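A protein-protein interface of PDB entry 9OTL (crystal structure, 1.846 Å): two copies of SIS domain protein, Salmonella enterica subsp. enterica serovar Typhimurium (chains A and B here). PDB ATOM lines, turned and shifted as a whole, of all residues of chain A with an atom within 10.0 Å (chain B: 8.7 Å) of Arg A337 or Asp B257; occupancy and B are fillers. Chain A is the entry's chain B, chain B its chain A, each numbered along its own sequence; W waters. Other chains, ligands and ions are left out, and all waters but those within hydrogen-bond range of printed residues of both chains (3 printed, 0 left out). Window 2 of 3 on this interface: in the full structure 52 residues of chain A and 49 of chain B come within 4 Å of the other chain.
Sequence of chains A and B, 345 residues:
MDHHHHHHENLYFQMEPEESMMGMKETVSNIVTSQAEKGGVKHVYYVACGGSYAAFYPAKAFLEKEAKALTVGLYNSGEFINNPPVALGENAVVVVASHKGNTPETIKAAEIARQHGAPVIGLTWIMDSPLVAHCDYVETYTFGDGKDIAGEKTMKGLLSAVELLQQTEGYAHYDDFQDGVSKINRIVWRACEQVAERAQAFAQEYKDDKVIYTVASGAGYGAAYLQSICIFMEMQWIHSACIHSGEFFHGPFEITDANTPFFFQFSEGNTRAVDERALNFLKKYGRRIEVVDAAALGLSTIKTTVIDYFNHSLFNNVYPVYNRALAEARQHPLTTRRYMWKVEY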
ATOM      1  N   LYS A 210     -12.597   4.643  -4.302  1.00  0.00           N
ATOM      2  CA  LYS A 210     -13.676   3.771  -3.869  1.00  0.00           C
ATOM      3  C   LYS A 210     -14.722   4.491  -2.992  1.00  0.00           C
ATOM      4  O   LYS A 210     -15.865   4.086  -2.981  1.00  0.00           O
ATOM      5  CB  LYS A 210     -12.999   2.681  -3.025  1.00  0.00           C
ATOM      6  CG  LYS A 210     -12.554   1.480  -3.807  1.00  0.00           C
ATOM      7  CD  LYS A 210     -12.307   0.270  -2.920  1.00  0.00           C
ATOM      8  CE  LYS A 210     -12.713  -0.950  -3.694  1.00  0.00           C
ATOM      9  NZ  LYS A 210     -12.322  -2.205  -3.051  1.00  0.00           N
ATOM     10  N   PHE A 232     -22.332   7.280  -3.722  1.00  0.00           N
ATOM     11  CA  PHE A 232     -22.395   5.939  -3.197  1.00  0.00           C
ATOM     12  C   PHE A 232     -22.953   5.025  -4.288  1.00  0.00           C
ATOM     13  O   PHE A 232     -22.428   3.910  -4.481  1.00  0.00           O
ATOM     14  CB  PHE A 232     -23.154   5.899  -1.860  1.00  0.00           C
ATOM     15  CG  PHE A 232     -23.357   4.452  -1.465  1.00  0.00           C
ATOM     16  CD1 PHE A 232     -22.280   3.684  -1.030  1.00  0.00           C
ATOM     17  CD2 PHE A 232     -24.573   3.831  -1.662  1.00  0.00           C
ATOM     18  CE1 PHE A 232     -22.447   2.342  -0.748  1.00  0.00           C
ATOM     19  CE2 PHE A 232     -24.724   2.489  -1.339  1.00  0.00           C
ATOM     20  CZ  PHE A 232     -23.666   1.754  -0.903  1.00  0.00           C
ATOM     21  N   MET A 233     -23.946   5.517  -5.010  1.00  0.00           N
ATOM     22  CA  MET A 233     -24.560   4.694  -6.037  1.00  0.00           C
ATOM     23  C   MET A 233     -23.598   4.485  -7.202  1.00  0.00           C
ATOM     24  O   MET A 233     -23.686   3.471  -7.857  1.00  0.00           O
ATOM     25  CB  MET A 233     -25.853   5.302  -6.569  1.00  0.00           C
ATOM     26  CG  MET A 233     -27.009   5.132  -5.641  1.00  0.00           C
ATOM     27  SD  MET A 233     -28.428   6.174  -6.055  1.00  0.00           S
ATOM     28  CE  MET A 233     -29.033   5.160  -7.417  1.00  0.00           C
ATOM     29  N   GLU A 234     -22.625   5.376  -7.417  1.00  0.00           N
ATOM     30  CA  GLU A 234     -21.612   5.150  -8.437  1.00  0.00           C
ATOM     31  C   GLU A 234     -20.496   4.228  -7.938  1.00  0.00           C
ATOM     32  O   GLU A 234     -20.044   3.342  -8.671  1.00  0.00           O
ATOM     33  CB  GLU A 234     -21.045   6.465  -8.965  1.00  0.00           C
ATOM     34  CG  GLU A 234     -19.975   6.257 -10.042  1.00  0.00           C
ATOM     35  CD  GLU A 234     -20.371   5.321 -11.195  1.00  0.00           C
ATOM     36  OE1 GLU A 234     -21.533   5.439 -11.647  1.00  0.00           O
ATOM     37  OE2 GLU A 234     -19.543   4.467 -11.640  1.00  0.00           O
ATOM     38  N   MET A 235     -20.008   4.449  -6.715  1.00  0.00           N
ATOM     39  CA  MET A 235     -18.799   3.811  -6.242  1.00  0.00           C
ATOM     40  C   MET A 235     -19.142   2.453  -5.607  1.00  0.00           C
ATOM     41  O   MET A 235     -18.409   1.465  -5.713  1.00  0.00           O
ATOM     42  CB  MET A 235     -18.137   4.666  -5.153  1.00  0.00           C
ATOM     43  CG  MET A 235     -17.654   6.027  -5.622  1.00  0.00           C
ATOM     44  SD  MET A 235     -16.637   5.887  -7.104  1.00  0.00           S
ATOM     45  CE  MET A 235     -15.334   7.011  -6.583  1.00  0.00           C
ATOM     46  N   GLN A 236     -20.252   2.424  -4.889  1.00  0.00           N
ATOM     47  CA  GLN A 236     -20.833   1.200  -4.356  1.00  0.00           C
ATOM     48  C   GLN A 236     -19.887   0.461  -3.434  1.00  0.00           C
ATOM     49  O   GLN A 236     -19.763  -0.745  -3.522  1.00  0.00           O
ATOM     50  CB  GLN A 236     -21.273   0.264  -5.457  1.00  0.00           C
ATOM     51  CG  GLN A 236     -22.290   0.938  -6.342  1.00  0.00           C
ATOM     52  CD  GLN A 236     -22.998   0.024  -7.319  1.00  0.00           C
ATOM     53  OE1 GLN A 236     -23.817   0.484  -8.112  1.00  0.00           O
ATOM     54  NE2 GLN A 236     -22.709  -1.256  -7.278  1.00  0.00           N
ATOM     55  N   TRP A 237     -19.219   1.174  -2.533  1.00  0.00           N
ATOM     56  CA  TRP A 237     -18.377   0.443  -1.632  1.00  0.00           C
ATOM     57  C   TRP A 237     -18.840   0.646  -0.187  1.00  0.00           C
ATOM     58  O   TRP A 237     -19.331  -0.292   0.444  1.00  0.00           O
ATOM     59  CB  TRP A 237     -16.911   0.790  -1.900  1.00  0.00           C
ATOM     60  CG  TRP A 237     -15.967  -0.133  -1.190  1.00  0.00           C
ATOM     61  CD1 TRP A 237     -15.176   0.197  -0.131  1.00  0.00           C
ATOM     62  CD2 TRP A 237     -15.768  -1.549  -1.410  1.00  0.00           C
ATOM     63  NE1 TRP A 237     -14.476  -0.900   0.306  1.00  0.00           N
ATOM     64  CE2 TRP A 237     -14.827  -1.990  -0.443  1.00  0.00           C
ATOM     65  CE3 TRP A 237     -16.286  -2.485  -2.309  1.00  0.00           C
ATOM     66  CZ2 TRP A 237     -14.374  -3.312  -0.372  1.00  0.00           C
ATOM     67  CZ3 TRP A 237     -15.855  -3.805  -2.223  1.00  0.00           C
ATOM     68  CH2 TRP A 237     -14.911  -4.211  -1.273  1.00  0.00           C
ATOM     69  N   ILE A 238     -18.602   1.847   0.352  1.00  0.00           N
ATOM     70  CA  ILE A 238     -19.046   2.248   1.679  1.00  0.00           C
ATOM     71  C   ILE A 238     -19.751   3.586   1.545  1.00  0.00           C
ATOM     72  O   ILE A 238     -19.259   4.499   0.857  1.00  0.00           O
ATOM     73  CB  ILE A 238     -17.853   2.308   2.651  1.00  0.00           C
ATOM     74  CG1 ILE A 238     -17.342   0.904   2.965  1.00  0.00           C
ATOM     75  CG2 ILE A 238     -18.248   3.078   3.928  1.00  0.00           C
ATOM     76  CD1 ILE A 238     -15.901   0.818   3.398  1.00  0.00           C
ATOM     77  N   HIS A 239     -20.925   3.697   2.162  1.00  0.00           N
ATOM     78  CA  HIS A 239     -21.606   4.983   2.237  1.00  0.00           C
ATOM     79  C   HIS A 239     -20.981   5.819   3.353  1.00  0.00           C
ATOM     80  O   HIS A 239     -21.073   5.492   4.517  1.00  0.00           O
ATOM     81  CB  HIS A 239     -23.106   4.831   2.410  1.00  0.00           C
ATOM     82  CG  HIS A 239     -23.812   6.126   2.366  1.00  0.00           C
ATOM     83  ND1 HIS A 239     -25.081   6.311   2.886  1.00  0.00           N
ATOM     84  CD2 HIS A 239     -23.425   7.313   1.822  1.00  0.00           C
ATOM     85  CE1 HIS A 239     -25.433   7.575   2.669  1.00  0.00           C
ATOM     86  NE2 HIS A 239     -24.458   8.197   2.014  1.00  0.00           N
ATOM     87  N   ARG A 330     -15.750   5.368 -15.813  1.00  0.00           N
ATOM     88  CA  ARG A 330     -15.569   4.143 -15.048  1.00  0.00           C
ATOM     89  C   ARG A 330     -16.247   2.978 -15.767  1.00  0.00           C
ATOM     90  O   ARG A 330     -17.437   3.014 -16.118  1.00  0.00           O
ATOM     91  CB  ARG A 330     -16.074   4.305 -13.618  1.00  0.00           C
ATOM     92  CG  ARG A 330     -15.092   5.102 -12.770  1.00  0.00           C
ATOM     93  CD  ARG A 330     -15.846   5.701 -11.620  1.00  0.00           C
ATOM     94  NE  ARG A 330     -16.682   4.724 -10.913  1.00  0.00           N
ATOM     95  CZ  ARG A 330     -16.182   3.891 -10.061  1.00  0.00           C
ATOM     96  NH1 ARG A 330     -14.904   3.994  -9.824  1.00  0.00           N
ATOM     97  NH2 ARG A 330     -16.941   3.004  -9.446  1.00  0.00           N
ATOM     98  N   HIS A 332     -16.130  -1.468 -15.598  1.00  0.00           N
ATOM     99  CA  HIS A 332     -15.878  -2.467 -14.583  1.00  0.00           C
ATOM    100  C   HIS A 332     -15.741  -3.801 -15.291  1.00  0.00           C
ATOM    101  O   HIS A 332     -16.495  -4.077 -16.218  1.00  0.00           O
ATOM    102  CB  HIS A 332     -17.026  -2.526 -13.569  1.00  0.00           C
ATOM    103  CG  HIS A 332     -17.475  -1.187 -13.089  1.00  0.00           C
ATOM    104  ND1 HIS A 332     -17.008  -0.585 -11.940  1.00  0.00           N
ATOM    105  CD2 HIS A 332     -18.369  -0.330 -13.637  1.00  0.00           C
ATOM    106  CE1 HIS A 332     -17.613   0.586 -11.807  1.00  0.00           C
ATOM    107  NE2 HIS A 332     -18.438   0.763 -12.829  1.00  0.00           N
ATOM    108  N   PRO A 333     -14.841  -4.678 -14.814  1.00  0.00           N
ATOM    109  CA  PRO A 333     -14.891  -6.056 -15.238  1.00  0.00           C
ATOM    110  C   PRO A 333     -16.245  -6.672 -14.934  1.00  0.00           C
ATOM    111  O   PRO A 333     -16.920  -6.259 -13.986  1.00  0.00           O
ATOM    112  CB  PRO A 333     -13.775  -6.742 -14.476  1.00  0.00           C
ATOM    113  CG  PRO A 333     -13.101  -5.657 -13.623  1.00  0.00           C
ATOM    114  CD  PRO A 333     -13.815  -4.381 -13.801  1.00  0.00           C
ATOM    115  N   LEU A 334     -16.628  -7.628 -15.779  1.00  0.00           N
ATOM    116  CA  LEU A 334     -17.872  -8.354 -15.632  1.00  0.00           C
ATOM    117  C   LEU A 334     -17.792  -9.259 -14.426  1.00  0.00           C
ATOM    118  O   LEU A 334     -18.849  -9.727 -14.015  1.00  0.00           O
ATOM    119  CB  LEU A 334     -18.253  -9.108 -16.898  1.00  0.00           C
ATOM    120  CG  LEU A 334     -18.548  -8.205 -18.101  1.00  0.00           C
ATOM    121  CD1 LEU A 334     -18.755  -9.008 -19.359  1.00  0.00           C
ATOM    122  CD2 LEU A 334     -19.781  -7.312 -17.834  1.00  0.00           C
ATOM    123  N   THR A 335     -16.584  -9.425 -13.832  1.00  0.00           N
ATOM    124  CA  THR A 335     -16.439 -10.170 -12.584  1.00  0.00           C
ATOM    125  C   THR A 335     -16.787  -9.333 -11.350  1.00  0.00           C
ATOM    126  O   THR A 335     -16.917  -9.917 -10.262  1.00  0.00           O
ATOM    127  CB  THR A 335     -15.041 -10.773 -12.422  1.00  0.00           C
ATOM    128  OG1 THR A 335     -14.099  -9.843 -12.950  1.00  0.00           O
ATOM    129  CG2 THR A 335     -15.000 -12.140 -13.071  1.00  0.00           C
ATOM    130  N   THR A 336     -16.980  -8.017 -11.519  1.00  0.00           N
ATOM    131  CA  THR A 336     -17.428  -7.126 -10.449  1.00  0.00           C
ATOM    132  C   THR A 336     -18.959  -7.002 -10.451  1.00  0.00           C
ATOM    133  O   THR A 336     -19.543  -6.532 -11.435  1.00  0.00           O
ATOM    134  CB  THR A 336     -16.781  -5.762 -10.670  1.00  0.00           C
ATOM    135  OG1 THR A 336     -15.417  -6.137 -10.584  1.00  0.00           O
ATOM    136  CG2 THR A 336     -17.231  -4.699  -9.679  1.00  0.00           C
ATOM    137  N   ARG A 337     -19.579  -7.391  -9.325  1.00  0.00           N
ATOM    138  CA  ARG A 337     -21.017  -7.252  -9.129  1.00  0.00           C
ATOM    139  C   ARG A 337     -21.330  -5.762  -9.030  1.00  0.00           C
ATOM    140  O   ARG A 337     -20.617  -5.032  -8.379  1.00  0.00           O
ATOM    141  CB  ARG A 337     -21.538  -8.019  -7.901  1.00  0.00           C
ATOM    142  CG  ARG A 337     -21.573  -9.541  -8.039  1.00  0.00           C
ATOM    143  CD  ARG A 337     -22.170 -10.295  -6.842  1.00  0.00           C
ATOM    144  NE  ARG A 337     -23.631 -10.196  -6.697  1.00  0.00           N
ATOM    145  CZ  ARG A 337     -24.588 -10.745  -7.476  1.00  0.00           C
ATOM    146  NH1 ARG A 337     -24.302 -11.576  -8.461  1.00  0.00           N
ATOM    147  NH2 ARG A 337     -25.864 -10.463  -7.263  1.00  0.00           N
ATOM    148  N   ARG A 338     -22.292  -5.314  -9.819  1.00  0.00           N
ATOM    149  CA  ARG A 338     -22.789  -3.956  -9.786  1.00  0.00           C
ATOM    150  C   ARG A 338     -24.258  -4.008  -9.372  1.00  0.00           C
ATOM    151  O   ARG A 338     -25.000  -4.907  -9.792  1.00  0.00           O
ATOM    152  CB  ARG A 338     -22.577  -3.280 -11.143  1.00  0.00           C
ATOM    153  CG  ARG A 338     -21.114  -3.091 -11.512  1.00  0.00           C
ATOM    154  CD  ARG A 338     -20.415  -2.079 -10.598  1.00  0.00           C
ATOM    155  NE  ARG A 338     -20.980  -0.741 -10.802  1.00  0.00           N
ATOM    156  CZ  ARG A 338     -20.647   0.367 -10.186  1.00  0.00           C
ATOM    157  NH1 ARG A 338     -19.823   0.367  -9.156  1.00  0.00           N
ATOM    158  NH2 ARG A 338     -21.190   1.496 -10.581  1.00  0.00           N
ATOM    159  N   TYR A 339     -24.683  -2.990  -8.608  1.00  0.00           N
ATOM    160  CA  TYR A 339     -25.999  -2.991  -7.974  1.00  0.00           C
ATOM    161  C   TYR A 339     -26.786  -1.849  -8.587  1.00  0.00           C
ATOM    162  O   TYR A 339     -26.235  -0.869  -9.058  1.00  0.00           O
ATOM    163  CB  TYR A 339     -25.922  -2.963  -6.438  1.00  0.00           C
ATOM    164  CG  TYR A 339     -25.233  -4.204  -5.877  1.00  0.00           C
ATOM    165  CD1 TYR A 339     -25.911  -5.411  -5.744  1.00  0.00           C
ATOM    166  CD2 TYR A 339     -23.889  -4.189  -5.552  1.00  0.00           C
ATOM    167  CE1 TYR A 339     -25.280  -6.550  -5.268  1.00  0.00           C
ATOM    168  CE2 TYR A 339     -23.228  -5.330  -5.136  1.00  0.00           C
ATOM    169  CZ  TYR A 339     -23.932  -6.514  -4.967  1.00  0.00           C
ATOM    170  OH  TYR A 339     -23.280  -7.620  -4.500  1.00  0.00           O
ATOM    171  N   MET A 340     -28.090  -2.063  -8.671  1.00  0.00           N
ATOM    172  CA  MET A 340     -29.051  -1.048  -9.011  1.00  0.00           C
ATOM    173  C   MET A 340     -30.231  -1.130  -8.045  1.00  0.00           C
ATOM    174  O   MET A 340     -30.495  -2.175  -7.406  1.00  0.00           O
ATOM    175  CB  MET A 340     -29.517  -1.192 -10.453  1.00  0.00           C
ATOM    176  CG  MET A 340     -30.092  -2.543 -10.806  1.00  0.00           C
ATOM    177  SD  MET A 340     -30.445  -2.597 -12.584  1.00  0.00           S
ATOM    178  CE  MET A 340     -30.774  -4.359 -12.533  1.00  0.00           C
ATOM    179  N   TRP A 341     -30.929   0.019  -7.964  1.00  0.00           N
ATOM    180  CA  TRP A 341     -32.010   0.254  -7.016  1.00  0.00           C
ATOM    181  C   TRP A 341     -33.114   1.022  -7.707  1.00  0.00           C
ATOM    182  O   TRP A 341     -32.821   1.755  -8.630  1.00  0.00           O
ATOM    183  CB  TRP A 341     -31.493   1.091  -5.830  1.00  0.00           C
ATOM    184  CG  TRP A 341     -30.392   0.445  -5.040  1.00  0.00           C
ATOM    185  CD1 TRP A 341     -30.542  -0.485  -4.054  1.00  0.00           C
ATOM    186  CD2 TRP A 341     -28.971   0.668  -5.171  1.00  0.00           C
ATOM    187  NE1 TRP A 341     -29.330  -0.817  -3.533  1.00  0.00           N
ATOM    188  CE2 TRP A 341     -28.347  -0.135  -4.194  1.00  0.00           C
ATOM    189  CE3 TRP A 341     -28.179   1.481  -5.990  1.00  0.00           C
ATOM    190  CZ2 TRP A 341     -26.967  -0.166  -4.020  1.00  0.00           C
ATOM    191  CZ3 TRP A 341     -26.809   1.448  -5.814  1.00  0.00           C
ATOM    192  CH2 TRP A 341     -26.216   0.660  -4.835  1.00  0.00           C
ATOM    193  N   PHE B 253     -29.474   1.087  -0.840  1.00  0.00           N
ATOM    194  CA  PHE B 253     -29.222   0.437   0.429  1.00  0.00           C
ATOM    195  C   PHE B 253     -27.717   0.215   0.550  1.00  0.00           C
ATOM    196  O   PHE B 253     -27.023  -0.073  -0.430  1.00  0.00           O
ATOM    197  CB  PHE B 253     -29.939  -0.922   0.547  1.00  0.00           C
ATOM    198  CG  PHE B 253     -31.382  -0.970   0.076  1.00  0.00           C
ATOM    199  CD1 PHE B 253     -32.356  -0.138   0.633  1.00  0.00           C
ATOM    200  CD2 PHE B 253     -31.763  -1.859  -0.939  1.00  0.00           C
ATOM    201  CE1 PHE B 253     -33.671  -0.193   0.199  1.00  0.00           C
ATOM    202  CE2 PHE B 253     -33.080  -1.896  -1.390  1.00  0.00           C
ATOM    203  CZ  PHE B 253     -34.027  -1.047  -0.845  1.00  0.00           C
ATOM    204  N   GLU B 254     -27.240   0.291   1.786  1.00  0.00           N
ATOM    205  CA  GLU B 254     -25.827   0.180   2.108  1.00  0.00           C
ATOM    206  C   GLU B 254     -25.424  -1.289   2.217  1.00  0.00           C
ATOM    207  O   GLU B 254     -24.917  -1.704   3.233  1.00  0.00           O
ATOM    208  CB  GLU B 254     -25.535   0.871   3.439  1.00  0.00           C
ATOM    209  CG  GLU B 254     -25.535   2.382   3.326  1.00  0.00           C
ATOM    210  CD  GLU B 254     -26.897   3.014   3.419  1.00  0.00           C
ATOM    211  OE1 GLU B 254     -27.926   2.309   3.633  1.00  0.00           O
ATOM    212  OE2 GLU B 254     -26.874   4.255   3.394  1.00  0.00           O
ATOM    213  N   ILE B 255     -25.601  -2.031   1.126  1.00  0.00           N
ATOM    214  CA  ILE B 255     -25.368  -3.465   1.048  1.00  0.00           C
ATOM    215  C   ILE B 255     -24.569  -3.700  -0.228  1.00  0.00           C
ATOM    216  O   ILE B 255     -25.065  -3.490  -1.322  1.00  0.00           O
ATOM    217  CB  ILE B 255     -26.729  -4.174   1.033  1.00  0.00           C
ATOM    218  CG1 ILE B 255     -27.395  -4.113   2.419  1.00  0.00           C
ATOM    219  CG2 ILE B 255     -26.594  -5.614   0.537  1.00  0.00           C
ATOM    220  CD1 ILE B 255     -28.910  -4.105   2.357  1.00  0.00           C
ATOM    221  N   THR B 256     -23.283  -3.904  -0.051  1.00  0.00           N
ATOM    222  CA  THR B 256     -22.347  -4.037  -1.139  1.00  0.00           C
ATOM    223  C   THR B 256     -21.447  -5.198  -0.798  1.00  0.00           C
ATOM    224  O   THR B 256     -21.546  -5.774   0.274  1.00  0.00           O
ATOM    225  CB  THR B 256     -21.515  -2.758  -1.336  1.00  0.00           C
ATOM    226  OG1 THR B 256     -20.524  -2.690  -0.295  1.00  0.00           O
ATOM    227  CG2 THR B 256     -22.434  -1.573  -1.435  1.00  0.00           C
ATOM    228  N   ASP B 257     -20.460  -5.393  -1.650  1.00  0.00           N
ATOM    229  CA  ASP B 257     -19.493  -6.444  -1.479  1.00  0.00           C
ATOM    230  C   ASP B 257     -18.388  -6.046  -0.522  1.00  0.00           C
ATOM    231  O   ASP B 257     -17.488  -6.845  -0.294  1.00  0.00           O
ATOM    232  CB  ASP B 257     -19.010  -6.874  -2.851  1.00  0.00           C
ATOM    233  CG  ASP B 257     -20.116  -7.596  -3.608  1.00  0.00           C
ATOM    234  OD1 ASP B 257     -20.817  -8.440  -2.982  1.00  0.00           O
ATOM    235  OD2 ASP B 257     -20.331  -7.263  -4.771  1.00  0.00           O
ATOM    236  N   ALA B 258     -18.470  -4.864   0.079  1.00  0.00           N
ATOM    237  CA  ALA B 258     -17.577  -4.547   1.182  1.00  0.00           C
ATOM    238  C   ALA B 258     -17.956  -5.380   2.393  1.00  0.00           C
ATOM    239  O   ALA B 258     -17.143  -5.528   3.285  1.00  0.00           O
ATOM    240  CB  ALA B 258     -17.627  -3.077   1.508  1.00  0.00           C
ATOM    241  N   ASN B 259     -19.197  -5.897   2.421  1.00  0.00           N
ATOM    242  CA  ASN B 259     -19.758  -6.648   3.541  1.00  0.00           C
ATOM    243  C   ASN B 259     -19.549  -5.917   4.869  1.00  0.00           C
ATOM    244  O   ASN B 259     -19.237  -6.521   5.897  1.00  0.00           O
ATOM    245  CB  ASN B 259     -19.303  -8.106   3.482  1.00  0.00           C
ATOM    246  CG  ASN B 259     -19.796  -8.767   2.202  1.00  0.00           C
ATOM    247  OD1 ASN B 259     -20.953  -8.613   1.780  1.00  0.00           O
ATOM    248  ND2 ASN B 259     -18.899  -9.421   1.485  1.00  0.00           N
ATOM    249  N   THR B 260     -19.833  -4.611   4.871  1.00  0.00           N
ATOM    250  CA  THR B 260     -19.735  -3.819   6.091  1.00  0.00           C
ATOM    251  C   THR B 260     -20.783  -4.328   7.092  1.00  0.00           C
ATOM    252  O   THR B 260     -21.953  -4.544   6.740  1.00  0.00           O
ATOM    253  CB  THR B 260     -19.959  -2.345   5.754  1.00  0.00           C
ATOM    254  OG1 THR B 260     -19.090  -2.032   4.670  1.00  0.00           O
ATOM    255  CG2 THR B 260     -19.706  -1.441   6.949  1.00  0.00           C
ATOM    256  N   TYR B 285     -31.102 -10.085   4.168  1.00  0.00           N
ATOM    257  CA  TYR B 285     -29.993  -9.926   3.246  1.00  0.00           C
ATOM    258  C   TYR B 285     -28.761 -10.644   3.763  1.00  0.00           C
ATOM    259  O   TYR B 285     -27.701 -10.498   3.186  1.00  0.00           O
ATOM    260  CB  TYR B 285     -29.652  -8.458   2.970  1.00  0.00           C
ATOM    261  CG  TYR B 285     -30.338  -7.959   1.710  1.00  0.00           C
ATOM    262  CD1 TYR B 285     -29.758  -8.127   0.460  1.00  0.00           C
ATOM    263  CD2 TYR B 285     -31.582  -7.367   1.779  1.00  0.00           C
ATOM    264  CE1 TYR B 285     -30.409  -7.718  -0.700  1.00  0.00           C
ATOM    265  CE2 TYR B 285     -32.239  -6.938   0.636  1.00  0.00           C
ATOM    266  CZ  TYR B 285     -31.664  -7.139  -0.603  1.00  0.00           C
ATOM    267  OH  TYR B 285     -32.352  -6.659  -1.670  1.00  0.00           O
ATOM    268  N   ARG B 287     -26.912  -9.967   6.352  1.00  0.00           N
ATOM    269  CA  ARG B 287     -25.881  -9.047   6.814  1.00  0.00           C
ATOM    270  C   ARG B 287     -25.339  -9.466   8.178  1.00  0.00           C
ATOM    271  O   ARG B 287     -25.974 -10.243   8.902  1.00  0.00           O
ATOM    272  CB  ARG B 287     -26.492  -7.640   6.898  1.00  0.00           C
ATOM    273  CG  ARG B 287     -26.849  -7.063   5.536  1.00  0.00           C
ATOM    274  CD  ARG B 287     -25.599  -6.865   4.672  1.00  0.00           C
ATOM    275  NE  ARG B 287     -25.417  -7.936   3.695  1.00  0.00           N
ATOM    276  CZ  ARG B 287     -24.487  -7.926   2.723  1.00  0.00           C
ATOM    277  NH1 ARG B 287     -23.498  -7.058   2.712  1.00  0.00           N
ATOM    278  NH2 ARG B 287     -24.555  -8.803   1.744  1.00  0.00           N
ATOM    279  N   ARG B 288     -24.163  -8.927   8.522  1.00  0.00           N
ATOM    280  CA  ARG B 288     -23.593  -9.073   9.857  1.00  0.00           C
ATOM    281  C   ARG B 288     -24.104  -7.922  10.711  1.00  0.00           C
ATOM    282  O   ARG B 288     -24.003  -6.758  10.303  1.00  0.00           O
ATOM    283  CB  ARG B 288     -22.069  -9.132   9.754  1.00  0.00           C
ATOM    284  CG  ARG B 288     -21.628 -10.128   8.687  1.00  0.00           C
ATOM    285  CD  ARG B 288     -20.229  -9.927   8.076  1.00  0.00           C
ATOM    286  NE  ARG B 288     -19.212  -9.979   9.125  1.00  0.00           N
ATOM    287  CZ  ARG B 288     -18.206  -9.126   9.213  1.00  0.00           C
ATOM    288  NH1 ARG B 288     -17.973  -8.269   8.242  1.00  0.00           N
ATOM    289  NH2 ARG B 288     -17.423  -9.139  10.254  1.00  0.00           N
HETATM  290  O   HOH W   1     -19.770  -3.581  -3.978  1.00  0.00           O
HETATM  291  O   HOH W   2     -18.447  -8.623  -7.230  1.00  0.00           O
HETATM  292  O   HOH W   3     -20.688  -0.892   2.604  1.00  0.00           O
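NE1 of Trp A341 lies close to N of Phe B253, at 3.3 Å.
The side-chain carboxylate (OD2) of Asp B257 is in hydrogen-bond range of the side-chain hydroxyl (OH) of Tyr A339.
OG1 of Thr B256 is in hydrogen-bond range of O of Trp A237 (2.8 Å).
The side-chain carboxylate (OE2) of Glu B254 is in hydrogen-bond range of a ring nitrogen (ND1) of His A239 (2.8 Å).
The backbone carbonyl oxygen (O) of Met A233 sits close to the side-chain amide oxygen (OE1) of Gln A236.
O of Asp B257 is in hydrogen-bond range of ND2 of Asn B259 (3.4 Å).
OG1 of Thr B256 lies within hydrogen-bond range of N of Ala B258, at 3.0 Å.
OE1 of Gln A236 lies close to O of Tyr A339, 2.9 Å away.
The backbone carbonyl oxygen (O) of Thr B256 is in hydrogen-bond range of the guanidinium group (NH1) of Arg B287, at 3.4 Å.
OD1 of Asn B259 lies close to O of Thr B256, at 3.3 Å.
Among the printed residues, pairs that only touch across the chains: Trp A237 with Ala B258 (3.4 Å), Arg A337 with Asp B257 (3.4 Å), Gln A236 with Thr B256 (3.4 Å), Phe A232 with Phe B253 (3.6 Å), Phe A232 with Thr B256 (3.6 Å), Trp A237 with Asp B257 (3.8 Å) and Ile A238 with Thr B260 (3.8 Å).
Of chain B, only Asp B257 comes within 4 Å of Arg A337.
Printed residues of chain A within 4 Å of Asp B257: Trp A237, Arg A337 and Tyr A339.
No residue of chain B comes within 4 Å of Thr A336.
Of the printed residues of chain A, Thr B260 touches Ile A238.
Of the printed residues of chain B, Phe A232 touches Phe B253 (3.6 Å) and Thr B256 (3.6 Å).
The nearest residue of chain B that does not touch Arg A337 is Thr B256 (7.5 Å).
The nearest printed residue of chain B that does not touch Gln A236 is Asp B257 (5.1 Å).
Of the 11 printed residues of chain B, 6 touch a printed residue of chain A.
Printed residues of chain B that touch a printed residue of chain A: Phe B253, Glu B254, Thr B256, Asp B257, Ala B258 and Thr B260.
Of the 20 printed residues of chain A, 8 touch a printed residue of chain B.
Printed residues of chain A that touch a printed residue of chain B: Phe A232, Gln A236, Trp A237, Ile A238, His A239, Arg A337, Tyr A339 and Trp A341.
Hydrophobic or aromatic side chains of chain A that line the printed part of chain B: Phe A232, Trp A237, Ile A238, His A239, Tyr A339 and Trp A341.
Among the printed residues, 11 pairs touch across the chains.
No position is printed for both chains.
Of the 11 pairs that touch across the chains among the printed residues, none has its exchanged pair printed and touching as well.
Water W3 lies within hydrogen-bond range of the backbone carbonyl oxygen of Trp A237 (2.6 Å), the side-chain hydroxyl of Thr B260 (2.8 Å) and the side-chain hydroxyl of Thr B256 (3.4 Å).
Water W2 lies within hydrogen-bond range of the backbone NH (N) of Arg A337 (2.7 Å) and the side-chain carboxylate (OD2) of Asp B257 (3.4 Å).
Water W1 lies within hydrogen-bond range of the backbone carbonyl oxygen of Gln A236 (2.9 Å) and the backbone NH of Asp B257 (3.0 Å).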
